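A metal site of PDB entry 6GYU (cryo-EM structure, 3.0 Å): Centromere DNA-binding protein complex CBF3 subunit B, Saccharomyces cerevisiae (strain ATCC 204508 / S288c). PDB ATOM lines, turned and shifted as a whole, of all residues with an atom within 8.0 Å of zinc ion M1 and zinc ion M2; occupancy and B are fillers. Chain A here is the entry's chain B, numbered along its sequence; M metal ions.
Pro 29 touches zinc ion M2. Five residues have an atom within 4 Å of zinc ion M2: Cys 14, Pro 29, Cys 30, Cys 33 and Cys 42.
Zinc ion M2 is bound by the side-chain sulfur (SG) of Cys 30 (2.5 Å), the side-chain sulfur (SG) of Cys 42 (2.5 Å), the side-chain sulfur (SG) of Cys 33 (2.5 Å) and the side-chain sulfur (SG) of Cys 14 (2.6 Å). Zinc ion M2 has four donor atoms within binding distance.
Zinc ion M1 is bound by SG of Cys 30 (2.5 Å), SG of Cys 17 (2.5 Å), SG of Cys 24 (2.5 Å) and SG of Cys 14 (2.5 Å).
The backbone carbonyl oxygen (O) of Pro 29 lies close to the side-chain sulfur (SG) of Cys 42 (3.3 Å). The side-chain sulfur (SG) of Cys 17 sits close to the backbone carbonyl oxygen (O) of Lys 23 (3.7 Å). The backbone NH (N) of Val 22 lies within hydrogen-bond range of the backbone carbonyl oxygen (O) of Cys 17 (3.2 Å). N of Val 16 sits close to SG of Cys 14. The side-chain hydroxyl (OG1) of Thr 18 is in hydrogen-bond range of the backbone carbonyl oxygen (O) of Cys 14. O of Cys 33 is in hydrogen-bond range of N of Gln 38, at 2.9 Å.
Within 4 Å of zinc ion M1: Cys 14, Cys 17, Cys 24 and Cys 30. The nearest printed residue that does not touch zinc ion M1 is Cys 33 (4.4 Å).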
ATOM      1  N   SER A  10      10.182 -15.164   0.464  1.00  0.00           N
ATOM      2  CA  SER A  10       9.685 -14.760  -0.837  1.00  0.00           C
ATOM      3  C   SER A  10       8.487 -13.835  -0.675  1.00  0.00           C
ATOM      4  O   SER A  10       7.833 -13.804   0.374  1.00  0.00           O
ATOM      5  CB  SER A  10       9.302 -15.975  -1.677  1.00  0.00           C
ATOM      6  OG  SER A  10       8.191 -16.644  -1.118  1.00  0.00           O
ATOM      7  N   HIS A  12       5.648 -13.365  -3.087  1.00  0.00           N
ATOM      8  CA  HIS A  12       4.449 -14.083  -3.456  1.00  0.00           C
ATOM      9  C   HIS A  12       4.542 -15.536  -2.990  1.00  0.00           C
ATOM     10  O   HIS A  12       5.628 -16.066  -2.772  1.00  0.00           O
ATOM     11  CB  HIS A  12       4.260 -14.023  -4.974  1.00  0.00           C
ATOM     12  CG  HIS A  12       5.431 -14.551  -5.736  1.00  0.00           C
ATOM     13  ND1 HIS A  12       6.546 -13.781  -6.012  1.00  0.00           N
ATOM     14  CD2 HIS A  12       5.689 -15.777  -6.262  1.00  0.00           C
ATOM     15  CE1 HIS A  12       7.420 -14.503  -6.691  1.00  0.00           C
ATOM     16  NE2 HIS A  12       6.919 -15.715  -6.851  1.00  0.00           N
ATOM     17  N   PRO A  13       3.390 -16.195  -2.798  1.00  0.00           N
ATOM     18  CA  PRO A  13       3.411 -17.656  -2.633  1.00  0.00           C
ATOM     19  C   PRO A  13       3.908 -18.331  -3.893  1.00  0.00           C
ATOM     20  O   PRO A  13       3.714 -17.838  -5.007  1.00  0.00           O
ATOM     21  CB  PRO A  13       1.942 -17.997  -2.354  1.00  0.00           C
ATOM     22  CG  PRO A  13       1.372 -16.748  -1.790  1.00  0.00           C
ATOM     23  CD  PRO A  13       2.068 -15.625  -2.511  1.00  0.00           C
ATOM     24  N   CYS A  14       4.568 -19.479  -3.707  1.00  0.00           N
ATOM     25  CA  CYS A  14       5.268 -20.136  -4.797  1.00  0.00           C
ATOM     26  C   CYS A  14       4.286 -20.744  -5.795  1.00  0.00           C
ATOM     27  O   CYS A  14       3.082 -20.878  -5.535  1.00  0.00           O
ATOM     28  CB  CYS A  14       6.202 -21.223  -4.265  1.00  0.00           C
ATOM     29  SG  CYS A  14       5.346 -22.662  -3.598  1.00  0.00           S
ATOM     30  N   SER A  15       4.824 -21.105  -6.963  1.00  0.00           N
ATOM     31  CA  SER A  15       3.996 -21.636  -8.036  1.00  0.00           C
ATOM     32  C   SER A  15       3.469 -23.025  -7.712  1.00  0.00           C
ATOM     33  O   SER A  15       2.409 -23.411  -8.215  1.00  0.00           O
ATOM     34  CB  SER A  15       4.804 -21.672  -9.337  1.00  0.00           C
ATOM     35  OG  SER A  15       5.893 -22.566  -9.232  1.00  0.00           O
ATOM     36  N   VAL A  16       4.177 -23.785  -6.881  1.00  0.00           N
ATOM     37  CA  VAL A  16       3.748 -25.139  -6.543  1.00  0.00           C
ATOM     38  C   VAL A  16       2.542 -25.108  -5.621  1.00  0.00           C
ATOM     39  O   VAL A  16       1.579 -25.857  -5.822  1.00  0.00           O
ATOM     40  CB  VAL A  16       4.926 -25.919  -5.932  1.00  0.00           C
ATOM     41  CG1 VAL A  16       4.483 -27.316  -5.520  1.00  0.00           C
ATOM     42  CG2 VAL A  16       6.078 -25.988  -6.914  1.00  0.00           C
ATOM     43  N   CYS A  17       2.549 -24.234  -4.602  1.00  0.00           N
ATOM     44  CA  CYS A  17       1.429 -24.147  -3.686  1.00  0.00           C
ATOM     45  C   CYS A  17       0.192 -23.487  -4.306  1.00  0.00           C
ATOM     46  O   CYS A  17      -0.912 -23.689  -3.796  1.00  0.00           O
ATOM     47  CB  CYS A  17       1.836 -23.400  -2.422  1.00  0.00           C
ATOM     48  SG  CYS A  17       2.984 -24.315  -1.376  1.00  0.00           S
ATOM     49  N   THR A  18       0.358 -22.730  -5.388  1.00  0.00           N
ATOM     50  CA  THR A  18      -0.792 -22.272  -6.157  1.00  0.00           C
ATOM     51  C   THR A  18      -1.276 -23.318  -7.158  1.00  0.00           C
ATOM     52  O   THR A  18      -2.452 -23.319  -7.509  1.00  0.00           O
ATOM     53  CB  THR A  18      -0.456 -20.977  -6.904  1.00  0.00           C
ATOM     54  OG1 THR A  18       0.647 -21.191  -7.788  1.00  0.00           O
ATOM     55  CG2 THR A  18      -0.100 -19.878  -5.913  1.00  0.00           C
ATOM     56  N   ARG A  20      -1.390 -26.380  -6.285  1.00  0.00           N
ATOM     57  CA  ARG A  20      -2.013 -27.353  -5.401  1.00  0.00           C
ATOM     58  C   ARG A  20      -3.097 -26.739  -4.520  1.00  0.00           C
ATOM     59  O   ARG A  20      -3.890 -27.482  -3.923  1.00  0.00           O
ATOM     60  CB  ARG A  20      -0.913 -28.015  -4.543  1.00  0.00           C
ATOM     61  CG  ARG A  20      -1.255 -29.264  -3.751  1.00  0.00           C
ATOM     62  CD  ARG A  20       0.013 -29.848  -3.187  1.00  0.00           C
ATOM     63  NE  ARG A  20       0.679 -28.907  -2.281  1.00  0.00           N
ATOM     64  CZ  ARG A  20       1.936 -29.030  -1.881  1.00  0.00           C
ATOM     65  NH1 ARG A  20       2.677 -30.028  -2.316  1.00  0.00           N
ATOM     66  NH2 ARG A  20       2.464 -28.126  -1.067  1.00  0.00           N
ATOM     67  N   VAL A  22      -3.005 -24.927  -1.652  1.00  0.00           N
ATOM     68  CA  VAL A  22      -2.825 -25.097  -0.223  1.00  0.00           C
ATOM     69  C   VAL A  22      -2.204 -23.832   0.342  1.00  0.00           C
ATOM     70  O   VAL A  22      -1.941 -22.866  -0.383  1.00  0.00           O
ATOM     71  CB  VAL A  22      -1.964 -26.324   0.119  1.00  0.00           C
ATOM     72  CG1 VAL A  22      -2.641 -27.602  -0.359  1.00  0.00           C
ATOM     73  CG2 VAL A  22      -0.582 -26.192  -0.489  1.00  0.00           C
ATOM     74  N   LYS A  23      -1.978 -23.826   1.652  1.00  0.00           N
ATOM     75  CA  LYS A  23      -1.258 -22.739   2.277  1.00  0.00           C
ATOM     76  C   LYS A  23       0.208 -22.777   1.873  1.00  0.00           C
ATOM     77  O   LYS A  23       0.746 -23.844   1.572  1.00  0.00           O
ATOM     78  CB  LYS A  23      -1.412 -22.797   3.808  1.00  0.00           C
ATOM     79  CG  LYS A  23      -0.826 -24.028   4.497  1.00  0.00           C
ATOM     80  CD  LYS A  23       0.543 -23.774   5.126  1.00  0.00           C
ATOM     81  CE  LYS A  23       1.076 -25.003   5.851  1.00  0.00           C
ATOM     82  NZ  LYS A  23       2.431 -24.767   6.411  1.00  0.00           N
ATOM     83  N   CYS A  24       0.851 -21.616   1.872  1.00  0.00           N
ATOM     84  CA  CYS A  24       2.261 -21.513   1.515  1.00  0.00           C
ATOM     85  C   CYS A  24       3.051 -21.078   2.737  1.00  0.00           C
ATOM     86  O   CYS A  24       2.851 -19.975   3.257  1.00  0.00           O
ATOM     87  CB  CYS A  24       2.461 -20.537   0.367  1.00  0.00           C
ATOM     88  SG  CYS A  24       4.174 -20.395  -0.197  1.00  0.00           S
ATOM     89  N   ASP A  25       3.946 -21.946   3.199  1.00  0.00           N
ATOM     90  CA  ASP A  25       4.948 -21.552   4.170  1.00  0.00           C
ATOM     91  C   ASP A  25       5.969 -20.696   3.439  1.00  0.00           C
ATOM     92  O   ASP A  25       6.975 -21.207   2.938  1.00  0.00           O
ATOM     93  CB  ASP A  25       5.611 -22.769   4.810  1.00  0.00           C
ATOM     94  CG  ASP A  25       6.620 -22.398   5.872  1.00  0.00           C
ATOM     95  OD1 ASP A  25       6.208 -21.954   6.968  1.00  0.00           O
ATOM     96  OD2 ASP A  25       7.830 -22.561   5.627  1.00  0.00           O
ATOM     97  N   ARG A  26       5.705 -19.392   3.371  1.00  0.00           N
ATOM     98  CA  ARG A  26       6.287 -18.519   2.349  1.00  0.00           C
ATOM     99  C   ARG A  26       7.767 -18.243   2.629  1.00  0.00           C
ATOM    100  O   ARG A  26       8.137 -17.125   3.007  1.00  0.00           O
ATOM    101  CB  ARG A  26       5.481 -17.221   2.287  1.00  0.00           C
ATOM    102  CG  ARG A  26       5.711 -16.353   1.062  1.00  0.00           C
ATOM    103  CD  ARG A  26       4.888 -15.093   1.150  1.00  0.00           C
ATOM    104  NE  ARG A  26       3.460 -15.365   1.086  1.00  0.00           N
ATOM    105  CZ  ARG A  26       2.525 -14.451   1.315  1.00  0.00           C
ATOM    106  NH1 ARG A  26       1.245 -14.774   1.235  1.00  0.00           N
ATOM    107  NH2 ARG A  26       2.886 -13.210   1.629  1.00  0.00           N
ATOM    108  N   MET A  27       8.593 -19.256   2.469  1.00  0.00           N
ATOM    109  CA  MET A  27      10.044 -19.141   2.598  1.00  0.00           C
ATOM    110  C   MET A  27      10.661 -19.252   1.209  1.00  0.00           C
ATOM    111  O   MET A  27       9.967 -19.267   0.187  1.00  0.00           O
ATOM    112  CB  MET A  27      10.600 -20.230   3.519  1.00  0.00           C
ATOM    113  CG  MET A  27      10.078 -20.237   4.946  1.00  0.00           C
ATOM    114  SD  MET A  27      10.275 -18.709   5.875  1.00  0.00           S
ATOM    115  CE  MET A  27       8.572 -18.239   6.117  1.00  0.00           C
ATOM    116  N   ILE A  28      11.984 -19.312   1.181  1.00  0.00           N
ATOM    117  CA  ILE A  28      12.733 -19.745   0.011  1.00  0.00           C
ATOM    118  C   ILE A  28      13.569 -20.956   0.410  1.00  0.00           C
ATOM    119  O   ILE A  28      14.468 -20.819   1.231  1.00  0.00           O
ATOM    120  CB  ILE A  28      13.617 -18.640  -0.589  1.00  0.00           C
ATOM    121  CG1 ILE A  28      12.736 -17.568  -1.239  1.00  0.00           C
ATOM    122  CG2 ILE A  28      14.569 -19.193  -1.618  1.00  0.00           C
ATOM    123  CD1 ILE A  28      13.501 -16.390  -1.813  1.00  0.00           C
ATOM    124  N   PRO A  29      13.283 -22.157  -0.113  1.00  0.00           N
ATOM    125  CA  PRO A  29      12.217 -22.404  -1.105  1.00  0.00           C
ATOM    126  C   PRO A  29      10.786 -22.529  -0.549  1.00  0.00           C
ATOM    127  O   PRO A  29       9.926 -21.862  -1.108  1.00  0.00           O
ATOM    128  CB  PRO A  29      12.641 -23.740  -1.730  1.00  0.00           C
ATOM    129  CG  PRO A  29      13.435 -24.420  -0.674  1.00  0.00           C
ATOM    130  CD  PRO A  29      14.141 -23.345   0.086  1.00  0.00           C
ATOM    131  N   CYS A  30      10.600 -23.258   0.554  1.00  0.00           N
ATOM    132  CA  CYS A  30       9.351 -23.463   1.292  1.00  0.00           C
ATOM    133  C   CYS A  30       9.610 -24.354   2.486  1.00  0.00           C
ATOM    134  O   CYS A  30      10.680 -24.958   2.606  1.00  0.00           O
ATOM    135  CB  CYS A  30       8.241 -24.120   0.457  1.00  0.00           C
ATOM    136  SG  CYS A  30       7.116 -23.069  -0.487  1.00  0.00           S
ATOM    137  N   GLY A  31       8.625 -24.454   3.376  1.00  0.00           N
ATOM    138  CA  GLY A  31       8.582 -25.592   4.282  1.00  0.00           C
ATOM    139  C   GLY A  31       7.707 -26.696   3.726  1.00  0.00           C
ATOM    140  O   GLY A  31       7.858 -27.857   4.123  1.00  0.00           O
ATOM    141  N   ASN A  32       6.814 -26.358   2.798  1.00  0.00           N
ATOM    142  CA  ASN A  32       5.823 -27.284   2.271  1.00  0.00           C
ATOM    143  C   ASN A  32       6.315 -27.982   1.010  1.00  0.00           C
ATOM    144  O   ASN A  32       5.853 -29.081   0.679  1.00  0.00           O
ATOM    145  CB  ASN A  32       4.526 -26.529   1.999  1.00  0.00           C
ATOM    146  CG  ASN A  32       3.312 -27.428   1.938  1.00  0.00           C
ATOM    147  OD1 ASN A  32       3.404 -28.645   2.103  1.00  0.00           O
ATOM    148  ND2 ASN A  32       2.144 -26.832   1.707  1.00  0.00           N
ATOM    149  N   CYS A  33       7.269 -27.364   0.302  1.00  0.00           N
ATOM    150  CA  CYS A  33       7.874 -28.011  -0.858  1.00  0.00           C
ATOM    151  C   CYS A  33       9.165 -28.729  -0.482  1.00  0.00           C
ATOM    152  O   CYS A  33       9.521 -29.720  -1.122  1.00  0.00           O
ATOM    153  CB  CYS A  33       8.142 -26.991  -1.958  1.00  0.00           C
ATOM    154  SG  CYS A  33       6.645 -26.264  -2.664  1.00  0.00           S
ATOM    155  N   ARG A  34       9.866 -28.244   0.538  1.00  0.00           N
ATOM    156  CA  ARG A  34      11.027 -28.953   1.069  1.00  0.00           C
ATOM    157  C   ARG A  34      10.598 -30.209   1.824  1.00  0.00           C
ATOM    158  O   ARG A  34      11.400 -31.152   1.946  1.00  0.00           O
ATOM    159  CB  ARG A  34      11.831 -28.006   1.959  1.00  0.00           C
ATOM    160  CG  ARG A  34      13.161 -28.514   2.470  1.00  0.00           C
ATOM    161  CD  ARG A  34      13.874 -27.398   3.210  1.00  0.00           C
ATOM    162  NE  ARG A  34      15.177 -27.783   3.746  1.00  0.00           N
ATOM    163  CZ  ARG A  34      15.357 -28.250   4.980  1.00  0.00           C
ATOM    164  NH1 ARG A  34      14.326 -28.376   5.792  1.00  0.00           N
ATOM    165  NH2 ARG A  34      16.574 -28.577   5.386  1.00  0.00           N
ATOM    166  N   GLN A  38      10.907 -31.191  -3.139  1.00  0.00           N
ATOM    167  CA  GLN A  38      10.772 -30.368  -4.336  1.00  0.00           C
ATOM    168  C   GLN A  38      11.593 -29.099  -4.232  1.00  0.00           C
ATOM    169  O   GLN A  38      11.116 -28.010  -4.585  1.00  0.00           O
ATOM    170  CB  GLN A  38       9.303 -30.063  -4.609  1.00  0.00           C
ATOM    171  CG  GLN A  38       8.492 -31.281  -4.990  1.00  0.00           C
ATOM    172  CD  GLN A  38       7.037 -30.968  -5.229  1.00  0.00           C
ATOM    173  OE1 GLN A  38       6.609 -29.833  -5.041  1.00  0.00           O
ATOM    174  NE2 GLN A  38       6.272 -31.959  -5.660  1.00  0.00           N
ATOM    175  N   ASP A  39      12.811 -29.219  -3.704  1.00  0.00           N
ATOM    176  CA  ASP A  39      13.698 -28.078  -3.490  1.00  0.00           C
ATOM    177  C   ASP A  39      14.045 -27.380  -4.802  1.00  0.00           C
ATOM    178  O   ASP A  39      13.886 -26.158  -4.930  1.00  0.00           O
ATOM    179  CB  ASP A  39      14.975 -28.550  -2.789  1.00  0.00           C
ATOM    180  CG  ASP A  39      15.932 -27.414  -2.485  1.00  0.00           C
ATOM    181  OD1 ASP A  39      15.691 -26.657  -1.528  1.00  0.00           O
ATOM    182  OD2 ASP A  39      16.940 -27.273  -3.222  1.00  0.00           O
ATOM    183  N   GLU A  41      12.613 -27.528  -7.708  1.00  0.00           N
ATOM    184  CA  GLU A  41      11.463 -27.119  -8.500  1.00  0.00           C
ATOM    185  C   GLU A  41      10.742 -25.903  -7.915  1.00  0.00           C
ATOM    186  O   GLU A  41       9.612 -25.618  -8.305  1.00  0.00           O
ATOM    187  CB  GLU A  41      10.484 -28.280  -8.652  1.00  0.00           C
ATOM    188  CG  GLU A  41      11.032 -29.456  -9.442  1.00  0.00           C
ATOM    189  CD  GLU A  41      11.258 -29.124 -10.910  1.00  0.00           C
ATOM    190  OE1 GLU A  41      10.486 -28.306 -11.461  1.00  0.00           O
ATOM    191  OE2 GLU A  41      12.206 -29.671 -11.507  1.00  0.00           O
ATOM    192  N   CYS A  42      11.374 -25.191  -6.978  1.00  0.00           N
ATOM    193  CA  CYS A  42      10.764 -24.019  -6.368  1.00  0.00           C
ATOM    194  C   CYS A  42      11.752 -22.852  -6.374  1.00  0.00           C
ATOM    195  O   CYS A  42      11.352 -21.689  -6.344  1.00  0.00           O
ATOM    196  CB  CYS A  42      10.314 -24.345  -4.942  1.00  0.00           C
ATOM    197  SG  CYS A  42       9.418 -23.026  -4.100  1.00  0.00           S
ATOM    198  N   MET A  43      13.053 -23.173  -6.433  1.00  0.00           N
ATOM    199  CA  MET A  43      14.078 -22.137  -6.426  1.00  0.00           C
ATOM    200  C   MET A  43      14.117 -21.353  -7.729  1.00  0.00           C
ATOM    201  O   MET A  43      14.526 -20.186  -7.736  1.00  0.00           O
ATOM    202  CB  MET A  43      15.447 -22.766  -6.174  1.00  0.00           C
ATOM    203  CG  MET A  43      15.631 -23.388  -4.802  1.00  0.00           C
ATOM    204  SD  MET A  43      15.485 -22.187  -3.481  1.00  0.00           S
ATOM    205  CE  MET A  43      16.969 -21.212  -3.754  1.00  0.00           C
HETATM  206 ZN    ZN M   1       4.778 -22.637  -1.119  1.00  0.00          ZN
HETATM  207 ZN    ZN M   2       7.444 -23.894  -2.825  1.00  0.00          ZN
